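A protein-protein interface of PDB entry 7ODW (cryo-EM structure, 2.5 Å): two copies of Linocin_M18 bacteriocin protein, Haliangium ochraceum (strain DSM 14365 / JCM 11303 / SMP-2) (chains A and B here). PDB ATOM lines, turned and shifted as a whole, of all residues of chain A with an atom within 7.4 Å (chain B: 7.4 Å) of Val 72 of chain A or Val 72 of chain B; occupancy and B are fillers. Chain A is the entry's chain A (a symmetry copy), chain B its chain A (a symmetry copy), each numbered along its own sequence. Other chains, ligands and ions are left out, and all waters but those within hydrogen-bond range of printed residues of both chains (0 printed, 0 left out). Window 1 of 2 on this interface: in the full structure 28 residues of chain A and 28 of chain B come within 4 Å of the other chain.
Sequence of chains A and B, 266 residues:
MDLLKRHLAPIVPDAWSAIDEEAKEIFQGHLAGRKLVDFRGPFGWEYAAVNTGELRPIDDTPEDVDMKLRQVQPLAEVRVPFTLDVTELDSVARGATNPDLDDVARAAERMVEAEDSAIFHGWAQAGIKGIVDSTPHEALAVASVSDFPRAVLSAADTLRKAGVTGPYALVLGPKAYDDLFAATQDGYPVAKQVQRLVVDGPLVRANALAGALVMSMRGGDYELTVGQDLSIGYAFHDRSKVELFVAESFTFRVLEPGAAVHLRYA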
ATOM      1  N   TYR A  47      28.598   7.729  -9.319  1.00  0.00           N
ATOM      2  CA  TYR A  47      27.950   8.275  -8.135  1.00  0.00           C
ATOM      3  C   TYR A  47      27.475   9.688  -8.447  1.00  0.00           C
ATOM      4  O   TYR A  47      28.291  10.574  -8.703  1.00  0.00           O
ATOM      5  CB  TYR A  47      28.919   8.277  -6.956  1.00  0.00           C
ATOM      6  CG  TYR A  47      28.332   8.769  -5.658  1.00  0.00           C
ATOM      7  CD1 TYR A  47      27.820   7.883  -4.727  1.00  0.00           C
ATOM      8  CD2 TYR A  47      28.307  10.118  -5.355  1.00  0.00           C
ATOM      9  CE1 TYR A  47      27.293   8.327  -3.543  1.00  0.00           C
ATOM     10  CE2 TYR A  47      27.779  10.570  -4.176  1.00  0.00           C
ATOM     11  CZ  TYR A  47      27.274   9.671  -3.273  1.00  0.00           C
ATOM     12  OH  TYR A  47      26.748  10.120  -2.089  1.00  0.00           O
ATOM     13  N   ALA A  48      26.164   9.902  -8.409  1.00  0.00           N
ATOM     14  CA  ALA A  48      25.573  11.103  -8.981  1.00  0.00           C
ATOM     15  C   ALA A  48      25.217  12.171  -7.960  1.00  0.00           C
ATOM     16  O   ALA A  48      25.455  13.353  -8.211  1.00  0.00           O
ATOM     17  CB  ALA A  48      24.318  10.741  -9.774  1.00  0.00           C
ATOM     18  N   ALA A  49      24.630  11.802  -6.827  1.00  0.00           N
ATOM     19  CA  ALA A  49      24.138  12.808  -5.902  1.00  0.00           C
ATOM     20  C   ALA A  49      24.229  12.292  -4.479  1.00  0.00           C
ATOM     21  O   ALA A  49      24.305  11.086  -4.238  1.00  0.00           O
ATOM     22  CB  ALA A  49      22.697  13.207  -6.214  1.00  0.00           C
ATOM     23  N   VAL A  50      24.218  13.227  -3.545  1.00  0.00           N
ATOM     24  CA  VAL A  50      24.236  12.925  -2.124  1.00  0.00           C
ATOM     25  C   VAL A  50      22.807  12.920  -1.611  1.00  0.00           C
ATOM     26  O   VAL A  50      22.051  13.870  -1.843  1.00  0.00           O
ATOM     27  CB  VAL A  50      25.088  13.947  -1.360  1.00  0.00           C
ATOM     28  CG1 VAL A  50      24.864  13.809   0.124  1.00  0.00           C
ATOM     29  CG2 VAL A  50      26.539  13.753  -1.688  1.00  0.00           C
ATOM     30  N   ASN A  51      22.434  11.849  -0.924  1.00  0.00           N
ATOM     31  CA  ASN A  51      21.112  11.742  -0.330  1.00  0.00           C
ATOM     32  C   ASN A  51      21.080  12.541   0.964  1.00  0.00           C
ATOM     33  O   ASN A  51      21.655  12.120   1.971  1.00  0.00           O
ATOM     34  CB  ASN A  51      20.773  10.280  -0.075  1.00  0.00           C
ATOM     35  CG  ASN A  51      19.628  10.109   0.883  1.00  0.00           C
ATOM     36  OD1 ASN A  51      18.654  10.854   0.843  1.00  0.00           O
ATOM     37  ND2 ASN A  51      19.735   9.121   1.755  1.00  0.00           N
ATOM     38  N   THR A  52      20.416  13.691   0.939  1.00  0.00           N
ATOM     39  CA  THR A  52      20.330  14.514   2.134  1.00  0.00           C
ATOM     40  C   THR A  52      19.377  13.945   3.172  1.00  0.00           C
ATOM     41  O   THR A  52      19.582  14.178   4.366  1.00  0.00           O
ATOM     42  CB  THR A  52      19.897  15.931   1.774  1.00  0.00           C
ATOM     43  OG1 THR A  52      18.472  15.982   1.683  1.00  0.00           O
ATOM     44  CG2 THR A  52      20.487  16.342   0.455  1.00  0.00           C
ATOM     45  N   GLY A  53      18.353  13.209   2.756  1.00  0.00           N
ATOM     46  CA  GLY A  53      17.424  12.593   3.674  1.00  0.00           C
ATOM     47  C   GLY A  53      16.136  13.347   3.904  1.00  0.00           C
ATOM     48  O   GLY A  53      15.201  12.771   4.467  1.00  0.00           O
ATOM     49  N   GLU A  54      16.041  14.602   3.489  1.00  0.00           N
ATOM     50  CA  GLU A  54      14.825  15.367   3.701  1.00  0.00           C
ATOM     51  C   GLU A  54      13.762  15.014   2.672  1.00  0.00           C
ATOM     52  O   GLU A  54      13.997  14.287   1.709  1.00  0.00           O
ATOM     53  CB  GLU A  54      15.100  16.870   3.662  1.00  0.00           C
ATOM     54  CG  GLU A  54      15.899  17.424   4.831  1.00  0.00           C
ATOM     55  CD  GLU A  54      17.343  16.982   4.843  1.00  0.00           C
ATOM     56  OE1 GLU A  54      17.742  16.238   3.929  1.00  0.00           O
ATOM     57  OE2 GLU A  54      18.082  17.381   5.766  1.00  0.00           O
ATOM     58  N   LEU A  69       8.480  14.519  -2.172  1.00  0.00           N
ATOM     59  CA  LEU A  69       9.598  14.312  -3.080  1.00  0.00           C
ATOM     60  C   LEU A  69      10.902  14.281  -2.302  1.00  0.00           C
ATOM     61  O   LEU A  69      11.164  15.172  -1.494  1.00  0.00           O
ATOM     62  CB  LEU A  69       9.646  15.416  -4.131  1.00  0.00           C
ATOM     63  CG  LEU A  69      10.010  14.985  -5.548  1.00  0.00           C
ATOM     64  CD1 LEU A  69       9.497  13.595  -5.841  1.00  0.00           C
ATOM     65  CD2 LEU A  69       9.454  15.974  -6.540  1.00  0.00           C
ATOM     66  N   ARG A  70      11.719  13.267  -2.550  1.00  0.00           N
ATOM     67  CA  ARG A  70      13.016  13.198  -1.901  1.00  0.00           C
ATOM     68  C   ARG A  70      13.900  14.349  -2.360  1.00  0.00           C
ATOM     69  O   ARG A  70      13.747  14.877  -3.461  1.00  0.00           O
ATOM     70  CB  ARG A  70      13.694  11.868  -2.201  1.00  0.00           C
ATOM     71  CG  ARG A  70      13.110  10.702  -1.449  1.00  0.00           C
ATOM     72  CD  ARG A  70      13.319  10.852   0.036  1.00  0.00           C
ATOM     73  NE  ARG A  70      14.649  10.434   0.449  1.00  0.00           N
ATOM     74  CZ  ARG A  70      14.944   9.207   0.850  1.00  0.00           C
ATOM     75  NH1 ARG A  70      14.002   8.284   0.888  1.00  0.00           N
ATOM     76  NH2 ARG A  70      16.177   8.903   1.211  1.00  0.00           N
ATOM     77  N   GLN A  71      14.822  14.750  -1.494  1.00  0.00           N
ATOM     78  CA  GLN A  71      15.749  15.834  -1.782  1.00  0.00           C
ATOM     79  C   GLN A  71      17.156  15.274  -1.874  1.00  0.00           C
ATOM     80  O   GLN A  71      17.563  14.469  -1.032  1.00  0.00           O
ATOM     81  CB  GLN A  71      15.687  16.916  -0.710  1.00  0.00           C
ATOM     82  CG  GLN A  71      14.317  17.499  -0.526  1.00  0.00           C
ATOM     83  CD  GLN A  71      13.930  18.417  -1.653  1.00  0.00           C
ATOM     84  OE1 GLN A  71      14.334  19.576  -1.689  1.00  0.00           O
ATOM     85  NE2 GLN A  71      13.146  17.904  -2.589  1.00  0.00           N
ATOM     86  N   VAL A  72      17.890  15.692  -2.902  1.00  0.00           N
ATOM     87  CA  VAL A  72      19.256  15.247  -3.118  1.00  0.00           C
ATOM     88  C   VAL A  72      20.115  16.445  -3.484  1.00  0.00           C
ATOM     89  O   VAL A  72      19.620  17.508  -3.857  1.00  0.00           O
ATOM     90  CB  VAL A  72      19.357  14.173  -4.215  1.00  0.00           C
ATOM     91  CG1 VAL A  72      18.789  12.866  -3.723  1.00  0.00           C
ATOM     92  CG2 VAL A  72      18.635  14.635  -5.452  1.00  0.00           C
ATOM     93  N   GLN A  73      21.422  16.251  -3.371  1.00  0.00           N
ATOM     94  CA  GLN A  73      22.410  17.253  -3.761  1.00  0.00           C
ATOM     95  C   GLN A  73      23.232  16.685  -4.906  1.00  0.00           C
ATOM     96  O   GLN A  73      24.112  15.841  -4.677  1.00  0.00           O
ATOM     97  CB  GLN A  73      23.302  17.613  -2.577  1.00  0.00           C
ATOM     98  CG  GLN A  73      24.347  18.662  -2.860  1.00  0.00           C
ATOM     99  CD  GLN A  73      23.787  20.061  -2.839  1.00  0.00           C
ATOM    100  OE1 GLN A  73      22.577  20.259  -2.873  1.00  0.00           O
ATOM    101  NE2 GLN A  73      24.669  21.046  -2.773  1.00  0.00           N
ATOM    102  N   PRO A  74      22.963  17.071  -6.149  1.00  0.00           N
ATOM    103  CA  PRO A  74      23.715  16.499  -7.270  1.00  0.00           C
ATOM    104  C   PRO A  74      25.159  16.969  -7.269  1.00  0.00           C
ATOM    105  O   PRO A  74      25.450  18.141  -7.029  1.00  0.00           O
ATOM    106  CB  PRO A  74      22.963  17.008  -8.501  1.00  0.00           C
ATOM    107  CG  PRO A  74      22.175  18.155  -8.036  1.00  0.00           C
ATOM    108  CD  PRO A  74      21.896  17.978  -6.592  1.00  0.00           C
ATOM    109  N   LEU A  75      26.068  16.040  -7.552  1.00  0.00           N
ATOM    110  CA  LEU A  75      27.482  16.362  -7.606  1.00  0.00           C
ATOM    111  C   LEU A  75      27.787  17.244  -8.809  1.00  0.00           C
ATOM    112  O   LEU A  75      27.039  17.296  -9.783  1.00  0.00           O
ATOM    113  CB  LEU A  75      28.326  15.097  -7.691  1.00  0.00           C
ATOM    114  CG  LEU A  75      28.821  14.489  -6.388  1.00  0.00           C
ATOM    115  CD1 LEU A  75      27.661  13.997  -5.574  1.00  0.00           C
ATOM    116  CD2 LEU A  75      29.774  13.359  -6.671  1.00  0.00           C
ATOM    117  N   ARG A 253      28.570  19.765   1.582  1.00  0.00           N
ATOM    118  CA  ARG A 253      27.357  19.970   2.353  1.00  0.00           C
ATOM    119  C   ARG A 253      27.689  20.539   3.722  1.00  0.00           C
ATOM    120  O   ARG A 253      28.598  20.058   4.409  1.00  0.00           O
ATOM    121  CB  ARG A 253      26.595  18.664   2.523  1.00  0.00           C
ATOM    122  CG  ARG A 253      25.514  18.446   1.505  1.00  0.00           C
ATOM    123  CD  ARG A 253      24.849  17.123   1.748  1.00  0.00           C
ATOM    124  NE  ARG A 253      23.784  17.229   2.734  1.00  0.00           N
ATOM    125  CZ  ARG A 253      23.504  16.285   3.621  1.00  0.00           C
ATOM    126  NH1 ARG A 253      24.217  15.169   3.647  1.00  0.00           N
ATOM    127  NH2 ARG A 253      22.516  16.458   4.483  1.00  0.00           N
ATOM    128  N   TYR B  47      17.172   5.238   0.028  1.00  0.00           N
ATOM    129  CA  TYR B  47      17.480   5.382  -1.388  1.00  0.00           C
ATOM    130  C   TYR B  47      16.682   6.553  -1.944  1.00  0.00           C
ATOM    131  O   TYR B  47      15.451   6.508  -1.971  1.00  0.00           O
ATOM    132  CB  TYR B  47      17.146   4.094  -2.135  1.00  0.00           C
ATOM    133  CG  TYR B  47      17.481   4.111  -3.605  1.00  0.00           C
ATOM    134  CD1 TYR B  47      18.681   3.601  -4.066  1.00  0.00           C
ATOM    135  CD2 TYR B  47      16.590   4.621  -4.532  1.00  0.00           C
ATOM    136  CE1 TYR B  47      18.986   3.609  -5.402  1.00  0.00           C
ATOM    137  CE2 TYR B  47      16.889   4.635  -5.867  1.00  0.00           C
ATOM    138  CZ  TYR B  47      18.087   4.127  -6.298  1.00  0.00           C
ATOM    139  OH  TYR B  47      18.387   4.137  -7.635  1.00  0.00           O
ATOM    140  N   ALA B  48      17.377   7.589  -2.402  1.00  0.00           N
ATOM    141  CA  ALA B  48      16.743   8.874  -2.665  1.00  0.00           C
ATOM    142  C   ALA B  48      16.445   9.134  -4.132  1.00  0.00           C
ATOM    143  O   ALA B  48      15.372   9.647  -4.451  1.00  0.00           O
ATOM    144  CB  ALA B  48      17.618  10.007  -2.131  1.00  0.00           C
ATOM    145  N   ALA B  49      17.366   8.824  -5.037  1.00  0.00           N
ATOM    146  CA  ALA B  49      17.177   9.201  -6.426  1.00  0.00           C
ATOM    147  C   ALA B  49      17.841   8.185  -7.335  1.00  0.00           C
ATOM    148  O   ALA B  49      18.727   7.437  -6.919  1.00  0.00           O
ATOM    149  CB  ALA B  49      17.735  10.593  -6.716  1.00  0.00           C
ATOM    150  N   VAL B  50      17.396   8.174  -8.579  1.00  0.00           N
ATOM    151  CA  VAL B  50      17.951   7.313  -9.610  1.00  0.00           C
ATOM    152  C   VAL B  50      18.997   8.096 -10.384  1.00  0.00           C
ATOM    153  O   VAL B  50      18.735   9.212 -10.846  1.00  0.00           O
ATOM    154  CB  VAL B  50      16.848   6.801 -10.545  1.00  0.00           C
ATOM    155  CG1 VAL B  50      17.455   6.162 -11.769  1.00  0.00           C
ATOM    156  CG2 VAL B  50      15.978   5.816  -9.821  1.00  0.00           C
ATOM    157  N   ASN B  51      20.182   7.517 -10.517  1.00  0.00           N
ATOM    158  CA  ASN B  51      21.254   8.133 -11.282  1.00  0.00           C
ATOM    159  C   ASN B  51      21.010   7.895 -12.764  1.00  0.00           C
ATOM    160  O   ASN B  51      21.193   6.778 -13.255  1.00  0.00           O
ATOM    161  CB  ASN B  51      22.597   7.558 -10.852  1.00  0.00           C
ATOM    162  CG  ASN B  51      23.690   7.835 -11.846  1.00  0.00           C
ATOM    163  OD1 ASN B  51      23.764   8.917 -12.420  1.00  0.00           O
ATOM    164  ND2 ASN B  51      24.553   6.855 -12.057  1.00  0.00           N
ATOM    165  N   THR B  52      20.594   8.936 -13.475  1.00  0.00           N
ATOM    166  CA  THR B  52      20.342   8.798 -14.900  1.00  0.00           C
ATOM    167  C   THR B  52      21.621   8.706 -15.716  1.00  0.00           C
ATOM    168  O   THR B  52      21.612   8.076 -16.777  1.00  0.00           O
ATOM    169  CB  THR B  52      19.502   9.965 -15.408  1.00  0.00           C
ATOM    170  OG1 THR B  52      20.358  11.070 -15.705  1.00  0.00           O
ATOM    171  CG2 THR B  52      18.502  10.385 -14.368  1.00  0.00           C
ATOM    172  N   GLY B  53      22.712   9.307 -15.255  1.00  0.00           N
ATOM    173  CA  GLY B  53      23.980   9.235 -15.942  1.00  0.00           C
ATOM    174  C   GLY B  53      24.315  10.416 -16.822  1.00  0.00           C
ATOM    175  O   GLY B  53      25.471  10.543 -17.234  1.00  0.00           O
ATOM    176  N   GLU B  54      23.362  11.287 -17.121  1.00  0.00           N
ATOM    177  CA  GLU B  54      23.638  12.429 -17.973  1.00  0.00           C
ATOM    178  C   GLU B  54      24.325  13.544 -17.201  1.00  0.00           C
ATOM    179  O   GLU B  54      24.468  13.505 -15.981  1.00  0.00           O
ATOM    180  CB  GLU B  54      22.359  12.963 -18.618  1.00  0.00           C
ATOM    181  CG  GLU B  54      21.729  12.065 -19.673  1.00  0.00           C
ATOM    182  CD  GLU B  54      21.127  10.800 -19.110  1.00  0.00           C
ATOM    183  OE1 GLU B  54      21.188  10.609 -17.883  1.00  0.00           O
ATOM    184  OE2 GLU B  54      20.588   9.995 -19.898  1.00  0.00           O
ATOM    185  N   LEU B  69      26.892  19.550 -14.207  1.00  0.00           N
ATOM    186  CA  LEU B  69      26.102  19.088 -13.075  1.00  0.00           C
ATOM    187  C   LEU B  69      25.478  17.740 -13.390  1.00  0.00           C
ATOM    188  O   LEU B  69      24.860  17.573 -14.441  1.00  0.00           O
ATOM    189  CB  LEU B  69      25.012  20.099 -12.735  1.00  0.00           C
ATOM    190  CG  LEU B  69      24.746  20.332 -11.251  1.00  0.00           C
ATOM    191  CD1 LEU B  69      26.015  20.189 -10.443  1.00  0.00           C
ATOM    192  CD2 LEU B  69      24.142  21.698 -11.050  1.00  0.00           C
ATOM    193  N   ARG B  70      25.631  16.787 -12.481  1.00  0.00           N
ATOM    194  CA  ARG B  70      25.007  15.489 -12.671  1.00  0.00           C
ATOM    195  C   ARG B  70      23.491  15.621 -12.643  1.00  0.00           C
ATOM    196  O   ARG B  70      22.936  16.529 -12.024  1.00  0.00           O
ATOM    197  CB  ARG B  70      25.466  14.514 -11.597  1.00  0.00           C
ATOM    198  CG  ARG B  70      26.872  14.011 -11.788  1.00  0.00           C
ATOM    199  CD  ARG B  70      26.991  13.194 -13.049  1.00  0.00           C
ATOM    200  NE  ARG B  70      26.543  11.824 -12.861  1.00  0.00           N
ATOM    201  CZ  ARG B  70      27.343  10.828 -12.515  1.00  0.00           C
ATOM    202  NH1 ARG B  70      28.628  11.055 -12.320  1.00  0.00           N
ATOM    203  NH2 ARG B  70      26.861   9.608 -12.364  1.00  0.00           N
ATOM    204  N   GLN B  71      22.820  14.712 -13.338  1.00  0.00           N
ATOM    205  CA  GLN B  71      21.367  14.697 -13.409  1.00  0.00           C
ATOM    206  C   GLN B  71      20.848  13.453 -12.711  1.00  0.00           C
ATOM    207  O   GLN B  71      21.377  12.357 -12.915  1.00  0.00           O
ATOM    208  CB  GLN B  71      20.881  14.724 -14.853  1.00  0.00           C
ATOM    209  CG  GLN B  71      21.381  15.907 -15.631  1.00  0.00           C
ATOM    210  CD  GLN B  71      20.687  17.182 -15.240  1.00  0.00           C
ATOM    211  OE1 GLN B  71      19.577  17.458 -15.686  1.00  0.00           O
ATOM    212  NE2 GLN B  71      21.334  17.973 -14.398  1.00  0.00           N
ATOM    213  N   VAL B  72      19.822  13.627 -11.883  1.00  0.00           N
ATOM    214  CA  VAL B  72      19.216  12.530 -11.148  1.00  0.00           C
ATOM    215  C   VAL B  72      17.705  12.656 -11.226  1.00  0.00           C
ATOM    216  O   VAL B  72      17.159  13.706 -11.564  1.00  0.00           O
ATOM    217  CB  VAL B  72      19.664  12.489  -9.677  1.00  0.00           C
ATOM    218  CG1 VAL B  72      21.099  12.037  -9.577  1.00  0.00           C
ATOM    219  CG2 VAL B  72      19.489  13.847  -9.051  1.00  0.00           C
ATOM    220  N   GLN B  73      17.034  11.558 -10.906  1.00  0.00           N
ATOM    221  CA  GLN B  73      15.577  11.509 -10.836  1.00  0.00           C
ATOM    222  C   GLN B  73      15.183  11.209  -9.399  1.00  0.00           C
ATOM    223  O   GLN B  73      15.287  10.054  -8.957  1.00  0.00           O
ATOM    224  CB  GLN B  73      15.032  10.444 -11.784  1.00  0.00           C
ATOM    225  CG  GLN B  73      13.529  10.323 -11.813  1.00  0.00           C
ATOM    226  CD  GLN B  73      12.877  11.385 -12.660  1.00  0.00           C
ATOM    227  OE1 GLN B  73      13.501  12.376 -13.025  1.00  0.00           O
ATOM    228  NE2 GLN B  73      11.611  11.180 -12.987  1.00  0.00           N
ATOM    229  N   PRO B  74      14.771  12.203  -8.621  1.00  0.00           N
ATOM    230  CA  PRO B  74      14.431  11.941  -7.219  1.00  0.00           C
ATOM    231  C   PRO B  74      13.162  11.113  -7.100  1.00  0.00           C
ATOM    232  O   PRO B  74      12.182  11.340  -7.810  1.00  0.00           O
ATOM    233  CB  PRO B  74      14.242  13.339  -6.629  1.00  0.00           C
ATOM    234  CG  PRO B  74      14.028  14.227  -7.777  1.00  0.00           C
ATOM    235  CD  PRO B  74      14.688  13.629  -8.961  1.00  0.00           C
ATOM    236  N   LEU B  75      13.186  10.152  -6.181  1.00  0.00           N
ATOM    237  CA  LEU B  75      12.030   9.303  -5.951  1.00  0.00           C
ATOM    238  C   LEU B  75      10.900  10.096  -5.311  1.00  0.00           C
ATOM    239  O   LEU B  75      11.104  11.149  -4.707  1.00  0.00           O
ATOM    240  CB  LEU B  75      12.388   8.130  -5.047  1.00  0.00           C
ATOM    241  CG  LEU B  75      12.831   6.836  -5.711  1.00  0.00           C
ATOM    242  CD1 LEU B  75      14.132   7.042  -6.429  1.00  0.00           C
ATOM    243  CD2 LEU B  75      12.972   5.747  -4.682  1.00  0.00           C
ATOM    244  N   ARG B 253      11.102   5.576 -15.030  1.00  0.00           N
ATOM    245  CA  ARG B 253      11.920   6.173 -16.070  1.00  0.00           C
ATOM    246  C   ARG B 253      11.627   5.525 -17.412  1.00  0.00           C
ATOM    247  O   ARG B 253      11.562   4.294 -17.524  1.00  0.00           O
ATOM    248  CB  ARG B 253      13.400   6.023 -15.751  1.00  0.00           C
ATOM    249  CG  ARG B 253      14.003   7.209 -15.059  1.00  0.00           C
ATOM    250  CD  ARG B 253      15.452   6.944 -14.768  1.00  0.00           C
ATOM    251  NE  ARG B 253      16.299   7.280 -15.903  1.00  0.00           N
ATOM    252  CZ  ARG B 253      17.381   6.595 -16.242  1.00  0.00           C
ATOM    253  NH1 ARG B 253      17.742   5.534 -15.537  1.00  0.00           N
ATOM    254  NH2 ARG B 253      18.100   6.968 -17.287  1.00  0.00           N
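N of Arg 70 of chain B is in hydrogen-bond range of O of Leu 75 of chain A (3.1 Å).
The backbone carbonyl oxygen (O) of Leu 75 of chain B sits at hydrogen-bond distance from the backbone NH (N) of Arg 70 of chain A.
The side-chain amide oxygen of Asn 51 of chain A lies within hydrogen-bond range of the backbone NH of Gly 53 of chain A (3.0 Å).
The side-chain amide oxygen (OD1) of Asn 51 of chain B lies within hydrogen-bond range of the guanidinium group (NH2) of Arg 70 of chain B, 3.2 Å away.
The side-chain amide oxygen (OD1) of Asn 51 of chain A is in hydrogen-bond range of the guanidinium group (NH2) of Arg 70 of chain A, 3.2 Å away.
The side-chain amide oxygen of Asn 51 of chain B lies within hydrogen-bond range of the backbone NH of Gly 53 of chain B, at 3.0 Å.
OH of Tyr 47 of chain A sits at hydrogen-bond distance from O of Ala 49 of chain A, at 3.4 Å.
The backbone NH of Leu 75 of chain A is in hydrogen-bond range of the backbone carbonyl oxygen of Ala 48 of chain A, at 2.8 Å.
Among the printed residues, pairs that only touch across the chains: Tyr 47 of chain A with Arg 70 of chain B (3.7 Å), Ala 48 of chain A with Asn 51 of chain B (3.3 Å), Ala 48 of chain A with Arg 70 of chain B (3.6 Å), Ala 48 of chain A with Val 72 of chain B (3.5 Å), Ala 49 of chain A with Val 72 of chain B (3.9 Å), Asn 51 of chain A with Ala 48 of chain B (3.3 Å), Leu 69 of chain A with Leu 75 of chain B (3.1 Å), Arg 70 of chain A with Tyr 47 of chain B (3.7 Å), Arg 70 of chain A with Ala 48 of chain B (3.6 Å), Arg 70 of chain A with Pro 74 of chain B (3.6 Å), Val 72 of chain A with Ala 48 of chain B (3.5 Å), Val 72 of chain A with Ala 49 of chain B (3.9 Å), Val 72 of chain A with Val 72 of chain B (3.8 Å), Pro 74 of chain A with Arg 70 of chain B (3.6 Å) and Leu 75 of chain A with Leu 69 of chain B (3.1 Å).
Val 72 of chain A touches three residues of chain B.
Of the printed residues of chain A, Ala 49 of chain B touches Val 72 (3.9 Å).
Of the printed residues of chain A, Leu 75 of chain B touches Leu 69 and Arg 70.
The nearest residue of chain B that does not touch Val 72 of chain A is Pro 74 of chain B (4.7 Å).
Of the 16 printed residues of chain B, 9 touch a printed residue of chain A.
Printed residues of chain B that touch a printed residue of chain A: Tyr 47, Ala 48, Ala 49, Asn 51, Leu 69, Arg 70, Val 72, Pro 74 and Leu 75.
Hydrophobic or aromatic side chains of chain A within 4 Å of the printed part of chain B: Ala 48, Ala 49, Leu 69, Val 72 and Pro 74.
Ala 49 of chain A touches Val 72 of chain B, and with the chains exchanged Val 72 of chain A touches Ala 49 of chain B.
Leu 69 of chain A touches Leu 75 of chain B, and with the chains exchanged Leu 75 of chain A touches Leu 69 of chain B.
Arg 70 of chain A touches Pro 74 of chain B, and with the chains exchanged Pro 74 of chain A touches Arg 70 of chain B.
Val 72 of chain A touches its own counterpart, Val 72 of chain B.
16 positions are printed for both chains.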
